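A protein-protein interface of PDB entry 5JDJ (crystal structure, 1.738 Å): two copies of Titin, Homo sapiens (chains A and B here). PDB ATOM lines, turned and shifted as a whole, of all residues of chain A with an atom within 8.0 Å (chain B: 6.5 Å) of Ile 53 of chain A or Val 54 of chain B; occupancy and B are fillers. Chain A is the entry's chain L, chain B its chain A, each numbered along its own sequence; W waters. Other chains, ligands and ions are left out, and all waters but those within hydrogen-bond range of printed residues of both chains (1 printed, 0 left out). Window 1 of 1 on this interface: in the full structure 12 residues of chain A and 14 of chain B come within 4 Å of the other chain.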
ATOM      1  N   PRO A  35     -34.694 -24.366  -0.726  1.00  0.00           N
ATOM      2  CA  PRO A  35     -33.508 -23.566  -1.029  1.00  0.00           C
ATOM      3  C   PRO A  35     -33.204 -22.574   0.086  1.00  0.00           C
ATOM      4  O   PRO A  35     -34.134 -22.023   0.663  1.00  0.00           O
ATOM      5  CB  PRO A  35     -33.890 -22.830  -2.317  1.00  0.00           C
ATOM      6  CG  PRO A  35     -35.368 -22.769  -2.305  1.00  0.00           C
ATOM      7  CD  PRO A  35     -35.848 -24.003  -1.564  1.00  0.00           C
ATOM      8  N   SER A  36     -31.930 -22.349   0.378  1.00  0.00           N
ATOM      9  CA  SER A  36     -31.565 -21.299   1.326  1.00  0.00           C
ATOM     10  C   SER A  36     -31.932 -19.918   0.787  1.00  0.00           C
ATOM     11  O   SER A  36     -31.695 -19.615  -0.391  1.00  0.00           O
ATOM     12  CB  SER A  36     -30.069 -21.331   1.635  1.00  0.00           C
ATOM     13  OG  SER A  36     -29.638 -22.629   2.034  1.00  0.00           O
ATOM     14  N   MET A  37     -32.504 -19.076   1.640  1.00  0.00           N
ATOM     15  CA  MET A  37     -32.673 -17.670   1.289  1.00  0.00           C
ATOM     16  C   MET A  37     -32.355 -16.807   2.497  1.00  0.00           C
ATOM     17  O   MET A  37     -33.044 -16.914   3.520  1.00  0.00           O
ATOM     18  CB  MET A  37     -34.091 -17.377   0.802  1.00  0.00           C
ATOM     19  CG  MET A  37     -34.268 -15.928   0.441  1.00  0.00           C
ATOM     20  SD  MET A  37     -35.744 -15.638  -0.550  1.00  0.00           S
ATOM     21  CE  MET A  37     -35.214 -14.194  -1.451  1.00  0.00           C
ATOM     22  N   TRP A  38     -31.311 -15.984   2.374  1.00  0.00           N
ATOM     23  CA  TRP A  38     -30.851 -15.136   3.469  1.00  0.00           C
ATOM     24  C   TRP A  38     -30.977 -13.641   3.161  1.00  0.00           C
ATOM     25  O   TRP A  38     -30.635 -13.189   2.065  1.00  0.00           O
ATOM     26  CB  TRP A  38     -29.390 -15.467   3.812  1.00  0.00           C
ATOM     27  CG  TRP A  38     -29.193 -16.821   4.428  1.00  0.00           C
ATOM     28  CD1 TRP A  38     -28.877 -17.975   3.783  1.00  0.00           C
ATOM     29  CD2 TRP A  38     -29.300 -17.152   5.819  1.00  0.00           C
ATOM     30  NE1 TRP A  38     -28.767 -19.012   4.691  1.00  0.00           N
ATOM     31  CE2 TRP A  38     -29.027 -18.529   5.943  1.00  0.00           C
ATOM     32  CE3 TRP A  38     -29.586 -16.414   6.970  1.00  0.00           C
ATOM     33  CZ2 TRP A  38     -29.038 -19.191   7.174  1.00  0.00           C
ATOM     34  CZ3 TRP A  38     -29.606 -17.083   8.201  1.00  0.00           C
ATOM     35  CH2 TRP A  38     -29.326 -18.453   8.285  1.00  0.00           C
ATOM     36  N   ILE A  45     -29.074 -10.915   0.630  1.00  0.00           N
ATOM     37  CA  ILE A  45     -27.637 -10.716   0.750  1.00  0.00           C
ATOM     38  C   ILE A  45     -26.995 -10.869  -0.631  1.00  0.00           C
ATOM     39  O   ILE A  45     -27.436 -11.681  -1.447  1.00  0.00           O
ATOM     40  CB  ILE A  45     -26.974 -11.696   1.744  1.00  0.00           C
ATOM     41  CG1 ILE A  45     -27.130 -13.139   1.270  1.00  0.00           C
ATOM     42  CG2 ILE A  45     -27.554 -11.537   3.159  1.00  0.00           C
ATOM     43  CD1 ILE A  45     -26.285 -14.121   2.066  1.00  0.00           C
ATOM     44  N   MET A  47     -24.316 -12.251  -2.806  1.00  0.00           N
ATOM     45  CA  MET A  47     -23.385 -13.353  -2.769  1.00  0.00           C
ATOM     46  C   MET A  47     -22.020 -12.873  -3.210  1.00  0.00           C
ATOM     47  O   MET A  47     -21.879 -12.119  -4.172  1.00  0.00           O
ATOM     48  CB  MET A  47     -23.893 -14.485  -3.647  1.00  0.00           C
ATOM     49  CG  MET A  47     -25.298 -14.894  -3.286  1.00  0.00           C
ATOM     50  SD  MET A  47     -25.373 -15.492  -1.595  1.00  0.00           S
ATOM     51  CE  MET A  47     -24.559 -17.056  -1.858  1.00  0.00           C
ATOM     52  N   SER A  48     -21.018 -13.295  -2.465  1.00  0.00           N
ATOM     53  CA  SER A  48     -19.640 -12.925  -2.722  1.00  0.00           C
ATOM     54  C   SER A  48     -18.840 -13.831  -1.835  1.00  0.00           C
ATOM     55  O   SER A  48     -19.423 -14.607  -1.078  1.00  0.00           O
ATOM     56  CB  SER A  48     -19.370 -11.455  -2.402  1.00  0.00           C
ATOM     57  OG  SER A  48     -19.262 -11.279  -1.004  1.00  0.00           O
ATOM     58  N   LYS A  50     -17.458 -13.265   0.691  1.00  0.00           N
ATOM     59  CA  LYS A  50     -17.699 -12.881   2.087  1.00  0.00           C
ATOM     60  C   LYS A  50     -18.654 -13.849   2.797  1.00  0.00           C
ATOM     61  O   LYS A  50     -18.532 -14.078   3.999  1.00  0.00           O
ATOM     62  CB  LYS A  50     -18.253 -11.461   2.150  1.00  0.00           C
ATOM     63  CG  LYS A  50     -18.561 -10.958   3.558  1.00  0.00           C
ATOM     64  CD  LYS A  50     -18.439  -9.452   3.607  1.00  0.00           C
ATOM     65  CE  LYS A  50     -18.427  -8.934   5.015  1.00  0.00           C
ATOM     66  NZ  LYS A  50     -17.199  -9.218   5.822  1.00  0.00           N
ATOM     67  N   PHE A  51     -19.594 -14.424   2.047  1.00  0.00           N
ATOM     68  CA  PHE A  51     -20.595 -15.320   2.626  1.00  0.00           C
ATOM     69  C   PHE A  51     -20.404 -16.774   2.183  1.00  0.00           C
ATOM     70  O   PHE A  51     -20.214 -17.034   1.004  1.00  0.00           O
ATOM     71  CB  PHE A  51     -22.007 -14.877   2.228  1.00  0.00           C
ATOM     72  CG  PHE A  51     -22.382 -13.500   2.705  1.00  0.00           C
ATOM     73  CD1 PHE A  51     -22.706 -13.279   4.034  1.00  0.00           C
ATOM     74  CD2 PHE A  51     -22.449 -12.447   1.821  1.00  0.00           C
ATOM     75  CE1 PHE A  51     -23.085 -12.020   4.476  1.00  0.00           C
ATOM     76  CE2 PHE A  51     -22.806 -11.178   2.255  1.00  0.00           C
ATOM     77  CZ  PHE A  51     -23.122 -10.969   3.586  1.00  0.00           C
ATOM     78  N   LYS A  52     -20.449 -17.713   3.115  1.00  0.00           N
ATOM     79  CA  LYS A  52     -20.594 -19.116   2.748  1.00  0.00           C
ATOM     80  C   LYS A  52     -22.004 -19.577   3.074  1.00  0.00           C
ATOM     81  O   LYS A  52     -22.489 -19.373   4.183  1.00  0.00           O
ATOM     82  CB  LYS A  52     -19.604 -20.023   3.484  1.00  0.00           C
ATOM     83  CG  LYS A  52     -18.160 -19.623   3.448  1.00  0.00           C
ATOM     84  CD  LYS A  52     -17.310 -20.724   4.086  1.00  0.00           C
ATOM     85  CE  LYS A  52     -15.863 -20.279   4.277  1.00  0.00           C
ATOM     86  NZ  LYS A  52     -15.031 -21.308   4.975  1.00  0.00           N
ATOM     87  N   ILE A  53     -22.654 -20.216   2.111  1.00  0.00           N
ATOM     88  CA  ILE A  53     -23.977 -20.776   2.327  1.00  0.00           C
ATOM     89  C   ILE A  53     -23.796 -22.271   2.419  1.00  0.00           C
ATOM     90  O   ILE A  53     -23.196 -22.869   1.530  1.00  0.00           O
ATOM     91  CB  ILE A  53     -24.956 -20.443   1.175  1.00  0.00           C
ATOM     92  CG1 ILE A  53     -25.043 -18.932   0.947  1.00  0.00           C
ATOM     93  CG2 ILE A  53     -26.338 -21.054   1.423  1.00  0.00           C
ATOM     94  CD1 ILE A  53     -25.792 -18.206   1.995  1.00  0.00           C
ATOM     95  N   VAL A  54     -24.293 -22.870   3.493  1.00  0.00           N
ATOM     96  CA  VAL A  54     -24.129 -24.303   3.712  1.00  0.00           C
ATOM     97  C   VAL A  54     -25.479 -24.952   3.954  1.00  0.00           C
ATOM     98  O   VAL A  54     -26.293 -24.425   4.710  1.00  0.00           O
ATOM     99  CB  VAL A  54     -23.205 -24.605   4.920  1.00  0.00           C
ATOM    100  CG1 VAL A  54     -22.958 -26.088   5.028  1.00  0.00           C
ATOM    101  CG2 VAL A  54     -21.887 -23.871   4.778  1.00  0.00           C
ATOM    102  N   VAL A  55     -25.724 -26.080   3.290  1.00  0.00           N
ATOM    103  CA  VAL A  55     -26.886 -26.906   3.597  1.00  0.00           C
ATOM    104  C   VAL A  55     -26.428 -28.340   3.842  1.00  0.00           C
ATOM    105  O   VAL A  55     -25.608 -28.885   3.116  1.00  0.00           O
ATOM    106  CB  VAL A  55     -27.929 -26.858   2.473  1.00  0.00           C
ATOM    107  CG1 VAL A  55     -29.189 -27.602   2.879  1.00  0.00           C
ATOM    108  CG2 VAL A  55     -28.282 -25.408   2.158  1.00  0.00           C
ATOM    109  N   GLN A  56     -26.939 -28.935   4.905  1.00  0.00           N
ATOM    110  CA  GLN A  56     -26.660 -30.323   5.211  1.00  0.00           C
ATOM    111  C   GLN A  56     -27.939 -30.920   5.779  1.00  0.00           C
ATOM    112  O   GLN A  56     -28.350 -30.572   6.873  1.00  0.00           O
ATOM    113  CB  GLN A  56     -25.498 -30.443   6.194  1.00  0.00           C
ATOM    114  CG  GLN A  56     -25.253 -31.852   6.677  1.00  0.00           C
ATOM    115  CD  GLN A  56     -24.085 -31.949   7.615  1.00  0.00           C
ATOM    116  OE1 GLN A  56     -23.681 -30.960   8.239  1.00  0.00           O
ATOM    117  NE2 GLN A  56     -23.533 -33.151   7.739  1.00  0.00           N
ATOM    118  N   LEU A  59     -30.505 -28.711   7.718  1.00  0.00           N
ATOM    119  CA  LEU A  59     -29.798 -27.629   8.403  1.00  0.00           C
ATOM    120  C   LEU A  59     -29.257 -26.617   7.395  1.00  0.00           C
ATOM    121  O   LEU A  59     -28.544 -26.986   6.462  1.00  0.00           O
ATOM    122  CB  LEU A  59     -28.655 -28.176   9.252  1.00  0.00           C
ATOM    123  CG  LEU A  59     -27.720 -27.100   9.821  1.00  0.00           C
ATOM    124  CD1 LEU A  59     -28.340 -26.385  11.021  1.00  0.00           C
ATOM    125  CD2 LEU A  59     -26.361 -27.690  10.186  1.00  0.00           C
ATOM    126  N   HIS A  60     -29.601 -25.347   7.584  1.00  0.00           N
ATOM    127  CA  HIS A  60     -29.146 -24.275   6.701  1.00  0.00           C
ATOM    128  C   HIS A  60     -28.273 -23.314   7.492  1.00  0.00           C
ATOM    129  O   HIS A  60     -28.662 -22.862   8.556  1.00  0.00           O
ATOM    130  CB  HIS A  60     -30.337 -23.530   6.083  1.00  0.00           C
ATOM    131  CG  HIS A  60     -31.161 -24.376   5.157  1.00  0.00           C
ATOM    132  ND1 HIS A  60     -31.223 -24.146   3.798  1.00  0.00           N
ATOM    133  CD2 HIS A  60     -31.950 -25.451   5.393  1.00  0.00           C
ATOM    134  CE1 HIS A  60     -32.020 -25.040   3.240  1.00  0.00           C
ATOM    135  NE2 HIS A  60     -32.470 -25.851   4.186  1.00  0.00           N
ATOM    136  N   GLN A  61     -27.080 -23.035   6.982  1.00  0.00           N
ATOM    137  CA  GLN A  61     -26.131 -22.183   7.684  1.00  0.00           C
ATOM    138  C   GLN A  61     -25.665 -21.014   6.813  1.00  0.00           C
ATOM    139  O   GLN A  61     -25.469 -21.154   5.608  1.00  0.00           O
ATOM    140  CB  GLN A  61     -24.944 -23.021   8.138  1.00  0.00           C
ATOM    141  CG  GLN A  61     -23.932 -22.313   8.996  1.00  0.00           C
ATOM    142  CD  GLN A  61     -22.856 -23.268   9.447  1.00  0.00           C
ATOM    143  OE1 GLN A  61     -22.565 -24.254   8.759  1.00  0.00           O
ATOM    144  NE2 GLN A  61     -22.277 -23.007  10.615  1.00  0.00           N
ATOM    145  N   LEU A  62     -25.514 -19.850   7.431  1.00  0.00           N
ATOM    146  CA  LEU A  62     -24.893 -18.711   6.768  1.00  0.00           C
ATOM    147  C   LEU A  62     -23.622 -18.378   7.525  1.00  0.00           C
ATOM    148  O   LEU A  62     -23.646 -18.196   8.751  1.00  0.00           O
ATOM    149  CB  LEU A  62     -25.833 -17.500   6.731  1.00  0.00           C
ATOM    150  CG  LEU A  62     -25.214 -16.192   6.208  1.00  0.00           C
ATOM    151  CD1 LEU A  62     -24.893 -16.280   4.719  1.00  0.00           C
ATOM    152  CD2 LEU A  62     -26.119 -14.987   6.474  1.00  0.00           C
ATOM    153  N   ILE A  63     -22.512 -18.327   6.803  1.00  0.00           N
ATOM    154  CA  ILE A  63     -21.224 -18.058   7.420  1.00  0.00           C
ATOM    155  C   ILE A  63     -20.716 -16.726   6.902  1.00  0.00           C
ATOM    156  O   ILE A  63     -20.614 -16.526   5.696  1.00  0.00           O
ATOM    157  CB  ILE A  63     -20.207 -19.174   7.128  1.00  0.00           C
ATOM    158  CG1 ILE A  63     -20.688 -20.509   7.711  1.00  0.00           C
ATOM    159  CG2 ILE A  63     -18.878 -18.815   7.723  1.00  0.00           C
ATOM    160  CD1 ILE A  63     -19.789 -21.669   7.415  1.00  0.00           C
ATOM    161  N   ILE A  64     -20.425 -15.799   7.815  1.00  0.00           N
ATOM    162  CA  ILE A  64     -19.995 -14.459   7.432  1.00  0.00           C
ATOM    163  C   ILE A  64     -18.515 -14.302   7.761  1.00  0.00           C
ATOM    164  O   ILE A  64     -18.114 -14.365   8.926  1.00  0.00           O
ATOM    165  CB  ILE A  64     -20.824 -13.367   8.147  1.00  0.00           C
ATOM    166  CG1 ILE A  64     -22.319 -13.598   7.922  1.00  0.00           C
ATOM    167  CG2 ILE A  64     -20.412 -11.975   7.678  1.00  0.00           C
ATOM    168  CD1 ILE A  64     -23.198 -12.588   8.617  1.00  0.00           C
ATOM    169  N   PHE A  77     -33.468 -15.771   7.713  1.00  0.00           N
ATOM    170  CA  PHE A  77     -33.667 -16.880   6.766  1.00  0.00           C
ATOM    171  C   PHE A  77     -35.149 -16.948   6.418  1.00  0.00           C
ATOM    172  O   PHE A  77     -35.995 -16.824   7.303  1.00  0.00           O
ATOM    173  CB  PHE A  77     -33.187 -18.201   7.370  1.00  0.00           C
ATOM    174  CG  PHE A  77     -33.329 -19.390   6.459  1.00  0.00           C
ATOM    175  CD1 PHE A  77     -32.287 -19.759   5.621  1.00  0.00           C
ATOM    176  CD2 PHE A  77     -34.482 -20.144   6.452  1.00  0.00           C
ATOM    177  CE1 PHE A  77     -32.402 -20.859   4.794  1.00  0.00           C
ATOM    178  CE2 PHE A  77     -34.608 -21.237   5.614  1.00  0.00           C
ATOM    179  CZ  PHE A  77     -33.555 -21.602   4.790  1.00  0.00           C
ATOM    180  N   SER B  36     -26.538 -24.739  -6.397  1.00  0.00           N
ATOM    181  CA  SER B  36     -25.754 -25.967  -6.483  1.00  0.00           C
ATOM    182  C   SER B  36     -26.617 -27.118  -6.952  1.00  0.00           C
ATOM    183  O   SER B  36     -27.758 -27.263  -6.513  1.00  0.00           O
ATOM    184  CB  SER B  36     -25.127 -26.322  -5.134  1.00  0.00           C
ATOM    185  OG  SER B  36     -23.861 -25.722  -4.970  1.00  0.00           O
ATOM    186  N   TRP B  38     -25.801 -31.329  -7.472  1.00  0.00           N
ATOM    187  CA  TRP B  38     -24.852 -32.428  -7.441  1.00  0.00           C
ATOM    188  C   TRP B  38     -25.518 -33.748  -7.755  1.00  0.00           C
ATOM    189  O   TRP B  38     -26.592 -34.040  -7.229  1.00  0.00           O
ATOM    190  CB  TRP B  38     -24.196 -32.522  -6.072  1.00  0.00           C
ATOM    191  CG  TRP B  38     -23.342 -31.349  -5.781  1.00  0.00           C
ATOM    192  CD1 TRP B  38     -23.732 -30.183  -5.197  1.00  0.00           C
ATOM    193  CD2 TRP B  38     -21.947 -31.212  -6.076  1.00  0.00           C
ATOM    194  NE1 TRP B  38     -22.664 -29.325  -5.105  1.00  0.00           N
ATOM    195  CE2 TRP B  38     -21.553 -29.933  -5.624  1.00  0.00           C
ATOM    196  CE3 TRP B  38     -20.987 -32.050  -6.664  1.00  0.00           C
ATOM    197  CZ2 TRP B  38     -20.245 -29.466  -5.745  1.00  0.00           C
ATOM    198  CZ3 TRP B  38     -19.693 -31.592  -6.776  1.00  0.00           C
ATOM    199  CH2 TRP B  38     -19.332 -30.304  -6.325  1.00  0.00           C
ATOM    200  N   LYS B  52     -22.706 -32.379   2.798  1.00  0.00           N
ATOM    201  CA  LYS B  52     -22.707 -30.931   3.036  1.00  0.00           C
ATOM    202  C   LYS B  52     -22.499 -30.214   1.717  1.00  0.00           C
ATOM    203  O   LYS B  52     -21.509 -30.464   1.033  1.00  0.00           O
ATOM    204  CB  LYS B  52     -21.603 -30.498   4.001  1.00  0.00           C
ATOM    205  CG  LYS B  52     -21.589 -31.137   5.356  1.00  0.00           C
ATOM    206  CD  LYS B  52     -20.613 -30.355   6.242  1.00  0.00           C
ATOM    207  CE  LYS B  52     -20.251 -31.099   7.522  1.00  0.00           C
ATOM    208  NZ  LYS B  52     -19.446 -30.239   8.442  1.00  0.00           N
ATOM    209  N   ILE B  53     -23.423 -29.332   1.360  1.00  0.00           N
ATOM    210  CA  ILE B  53     -23.297 -28.565   0.133  1.00  0.00           C
ATOM    211  C   ILE B  53     -22.916 -27.147   0.513  1.00  0.00           C
ATOM    212  O   ILE B  53     -23.563 -26.521   1.368  1.00  0.00           O
ATOM    213  CB  ILE B  53     -24.592 -28.562  -0.708  1.00  0.00           C
ATOM    214  CG1 ILE B  53     -24.885 -29.949  -1.290  1.00  0.00           C
ATOM    215  CG2 ILE B  53     -24.466 -27.589  -1.851  1.00  0.00           C
ATOM    216  CD1 ILE B  53     -25.480 -30.928  -0.311  1.00  0.00           C
ATOM    217  N   VAL B  54     -21.849 -26.651  -0.094  1.00  0.00           N
ATOM    218  CA  VAL B  54     -21.286 -25.360   0.299  1.00  0.00           C
ATOM    219  C   VAL B  54     -21.150 -24.483  -0.925  1.00  0.00           C
ATOM    220  O   VAL B  54     -20.640 -24.935  -1.948  1.00  0.00           O
ATOM    221  CB  VAL B  54     -19.896 -25.513   0.973  1.00  0.00           C
ATOM    222  CG1 VAL B  54     -19.406 -24.175   1.493  1.00  0.00           C
ATOM    223  CG2 VAL B  54     -19.941 -26.528   2.100  1.00  0.00           C
ATOM    224  N   VAL B  55     -21.644 -23.248  -0.841  1.00  0.00           N
ATOM    225  CA  VAL B  55     -21.373 -22.250  -1.879  1.00  0.00           C
ATOM    226  C   VAL B  55     -20.720 -21.037  -1.229  1.00  0.00           C
ATOM    227  O   VAL B  55     -21.227 -20.514  -0.237  1.00  0.00           O
ATOM    228  CB  VAL B  55     -22.637 -21.819  -2.617  1.00  0.00           C
ATOM    229  CG1 VAL B  55     -22.303 -20.801  -3.725  1.00  0.00           C
ATOM    230  CG2 VAL B  55     -23.331 -23.032  -3.199  1.00  0.00           C
ATOM    231  N   GLN B  56     -19.581 -20.621  -1.765  1.00  0.00           N
ATOM    232  CA  GLN B  56     -18.922 -19.402  -1.318  1.00  0.00           C
ATOM    233  C   GLN B  56     -18.518 -18.594  -2.536  1.00  0.00           C
ATOM    234  O   GLN B  56     -17.543 -18.936  -3.201  1.00  0.00           O
ATOM    235  CB  GLN B  56     -17.705 -19.704  -0.464  1.00  0.00           C
ATOM    236  CG  GLN B  56     -17.025 -18.427   0.019  1.00  0.00           C
ATOM    237  CD  GLN B  56     -15.850 -18.699   0.914  1.00  0.00           C
ATOM    238  OE1 GLN B  56     -15.386 -19.834   1.005  1.00  0.00           O
ATOM    239  NE2 GLN B  56     -15.347 -17.655   1.574  1.00  0.00           N
ATOM    240  N   LEU B  59     -17.477 -20.352  -5.704  1.00  0.00           N
ATOM    241  CA  LEU B  59     -16.968 -21.671  -5.353  1.00  0.00           C
ATOM    242  C   LEU B  59     -18.093 -22.571  -4.849  1.00  0.00           C
ATOM    243  O   LEU B  59     -18.842 -22.200  -3.937  1.00  0.00           O
ATOM    244  CB  LEU B  59     -15.861 -21.562  -4.300  1.00  0.00           C
ATOM    245  CG  LEU B  59     -15.264 -22.850  -3.719  1.00  0.00           C
ATOM    246  CD1 LEU B  59     -14.553 -23.701  -4.780  1.00  0.00           C
ATOM    247  CD2 LEU B  59     -14.311 -22.517  -2.575  1.00  0.00           C
ATOM    248  N   HIS B  60     -18.198 -23.748  -5.460  1.00  0.00           N
ATOM    249  CA  HIS B  60     -19.162 -24.764  -5.077  1.00  0.00           C
ATOM    250  C   HIS B  60     -18.472 -26.029  -4.597  1.00  0.00           C
ATOM    251  O   HIS B  60     -17.573 -26.544  -5.258  1.00  0.00           O
ATOM    252  CB  HIS B  60     -20.077 -25.099  -6.256  1.00  0.00           C
ATOM    253  CG  HIS B  60     -20.975 -23.974  -6.639  1.00  0.00           C
ATOM    254  ND1 HIS B  60     -22.337 -24.011  -6.437  1.00  0.00           N
ATOM    255  CD2 HIS B  60     -20.708 -22.773  -7.202  1.00  0.00           C
ATOM    256  CE1 HIS B  60     -22.871 -22.877  -6.852  1.00  0.00           C
ATOM    257  NE2 HIS B  60     -21.905 -22.110  -7.325  1.00  0.00           N
ATOM    258  N   GLN B  61     -18.907 -26.536  -3.453  1.00  0.00           N
ATOM    259  CA  GLN B  61     -18.250 -27.676  -2.836  1.00  0.00           C
ATOM    260  C   GLN B  61     -19.237 -28.720  -2.333  1.00  0.00           C
ATOM    261  O   GLN B  61     -20.274 -28.384  -1.757  1.00  0.00           O
ATOM    262  CB  GLN B  61     -17.379 -27.192  -1.678  1.00  0.00           C
ATOM    263  CG  GLN B  61     -16.784 -28.302  -0.835  1.00  0.00           C
ATOM    264  CD  GLN B  61     -15.931 -27.726   0.274  1.00  0.00           C
ATOM    265  OE1 GLN B  61     -16.316 -26.745   0.913  1.00  0.00           O
ATOM    266  NE2 GLN B  61     -14.758 -28.311   0.489  1.00  0.00           N
ATOM    267  N   LEU B  62     -18.906 -29.987  -2.552  1.00  0.00           N
ATOM    268  CA  LEU B  62     -19.668 -31.084  -1.984  1.00  0.00           C
ATOM    269  C   LEU B  62     -18.769 -31.766  -1.001  1.00  0.00           C
ATOM    270  O   LEU B  62     -17.658 -32.143  -1.358  1.00  0.00           O
ATOM    271  CB  LEU B  62     -20.117 -32.080  -3.044  1.00  0.00           C
ATOM    272  CG  LEU B  62     -20.835 -33.329  -2.520  1.00  0.00           C
ATOM    273  CD1 LEU B  62     -22.172 -32.957  -1.889  1.00  0.00           C
ATOM    274  CD2 LEU B  62     -21.070 -34.313  -3.666  1.00  0.00           C
ATOM    275  N   ILE B  63     -19.242 -31.909   0.234  1.00  0.00           N
ATOM    276  CA  ILE B  63     -18.505 -32.626   1.264  1.00  0.00           C
ATOM    277  C   ILE B  63     -19.272 -33.893   1.610  1.00  0.00           C
ATOM    278  O   ILE B  63     -20.465 -33.836   1.905  1.00  0.00           O
ATOM    279  CB  ILE B  63     -18.310 -31.758   2.529  1.00  0.00           C
ATOM    280  CG1 ILE B  63     -17.492 -30.508   2.193  1.00  0.00           C
ATOM    281  CG2 ILE B  63     -17.623 -32.564   3.618  1.00  0.00           C
ATOM    282  CD1 ILE B  63     -17.333 -29.545   3.364  1.00  0.00           C
HETATM  283  O   HOH W   1     -25.274 -24.434  -0.052  1.00  0.00           O
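The backbone carbonyl oxygen (O) of Val 54 of chain B sits at hydrogen-bond distance from the backbone NH (N) of Gln 61 of chain B. The backbone NH (N) of Ile 63 of chain B lies within hydrogen-bond range of the backbone carbonyl oxygen (O) of Lys 52 of chain B (2.8 Å). O of Lys 52 of chain A lies within hydrogen-bond range of N of Ile 63 of chain A. The backbone NH (N) of Gln 61 of chain A is in hydrogen-bond range of the backbone carbonyl oxygen (O) of Val 54 of chain A (2.8 Å).
The backbone carbonyl oxygen of Val 55 of chain B sits at hydrogen-bond distance from the backbone NH of Ile 53 of chain A. N of Ile 53 of chain B sits at hydrogen-bond distance from O of Val 55 of chain A (2.8 Å).
Among the printed residues, merely in contact across the chains: Phe 51 of chain A with Val 55 of chain B (3.8 Å), Phe 51 of chain A with Gln 56 of chain B (3.6 Å), Lys 52 of chain A with Val 55 of chain B (3.4 Å), Lys 52 of chain A with Gln 56 of chain B (3.3 Å), Ile 53 of chain A with Ile 53 of chain B (3.7 Å), Ile 53 of chain A with Val 54 of chain B (3.4 Å), Val 54 of chain A with Ile 53 of chain B (3.3 Å), Val 55 of chain A with Lys 52 of chain B (3.6 Å) and Gln 56 of chain A with Lys 52 of chain B (3.5 Å).
Lys 52 of chain A touches Val 55 of chain B, and with the chains exchanged Val 55 of chain A touches Lys 52 of chain B. Lys 52 of chain A touches Gln 56 of chain B, and with the chains exchanged Gln 56 of chain A touches Lys 52 of chain B. Ile 53 of chain B touches its own counterpart, Ile 53 of chain A. Ile 53 of chain A touches Val 55 of chain B, and with the chains exchanged Val 55 of chain A touches Ile 53 of chain B. Of the 11 pairs that touch across the chains among the printed residues, 9 have their exchanged pair printed and touching as well.
Water W1 bridges the backbone carbonyl oxygen (O) of Ile 53 of chain A (3.0 Å) and the backbone carbonyl oxygen (O) of Ile 53 of chain B (3.0 Å).
Printed residues of chain A that touch a printed residue of chain B: Phe 51, Lys 52, Ile 53, Val 54, Val 55 and Gln 56. Of the 12 printed residues of chain B, 5 touch a printed residue of chain A. Hydrophobic or aromatic side chains of chain B within 4 Å of the printed part of chain A: Ile 53. Among the printed residues, no Asp or Glu carboxylate lies within 4 Å of a Lys or Arg side-chain nitrogen of the other chain.
Met 37 of chain A touches none of the printed residues of chain B. Ile 53 of chain A touches three residues of chain B. Of the printed residues of chain B, Gln 56 of chain A touches Lys 52 (3.5 Å). Printed residues of chain A within 4 Å of Ile 53 of chain B: Ile 53 (3.7 Å), Val 54 (3.3 Å) and Val 55 (2.8 Å). Of chain A, only Ile 53 comes within 4 Å of Val 54 of chain B. Of the printed residues of chain A, Gln 56 of chain B touches Phe 51 (3.6 Å) and Lys 52 (3.3 Å). The nearest residue of chain B that does not touch Ile 53 of chain A is Gln 56 of chain B (5.0 Å). The nearest residue of chain A that does not touch Val 54 of chain B is Val 54 of chain A (4.1 Å). The nearest printed residue of chain B that does not touch Val 54 of chain A is Val 54 of chain B (4.1 Å).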
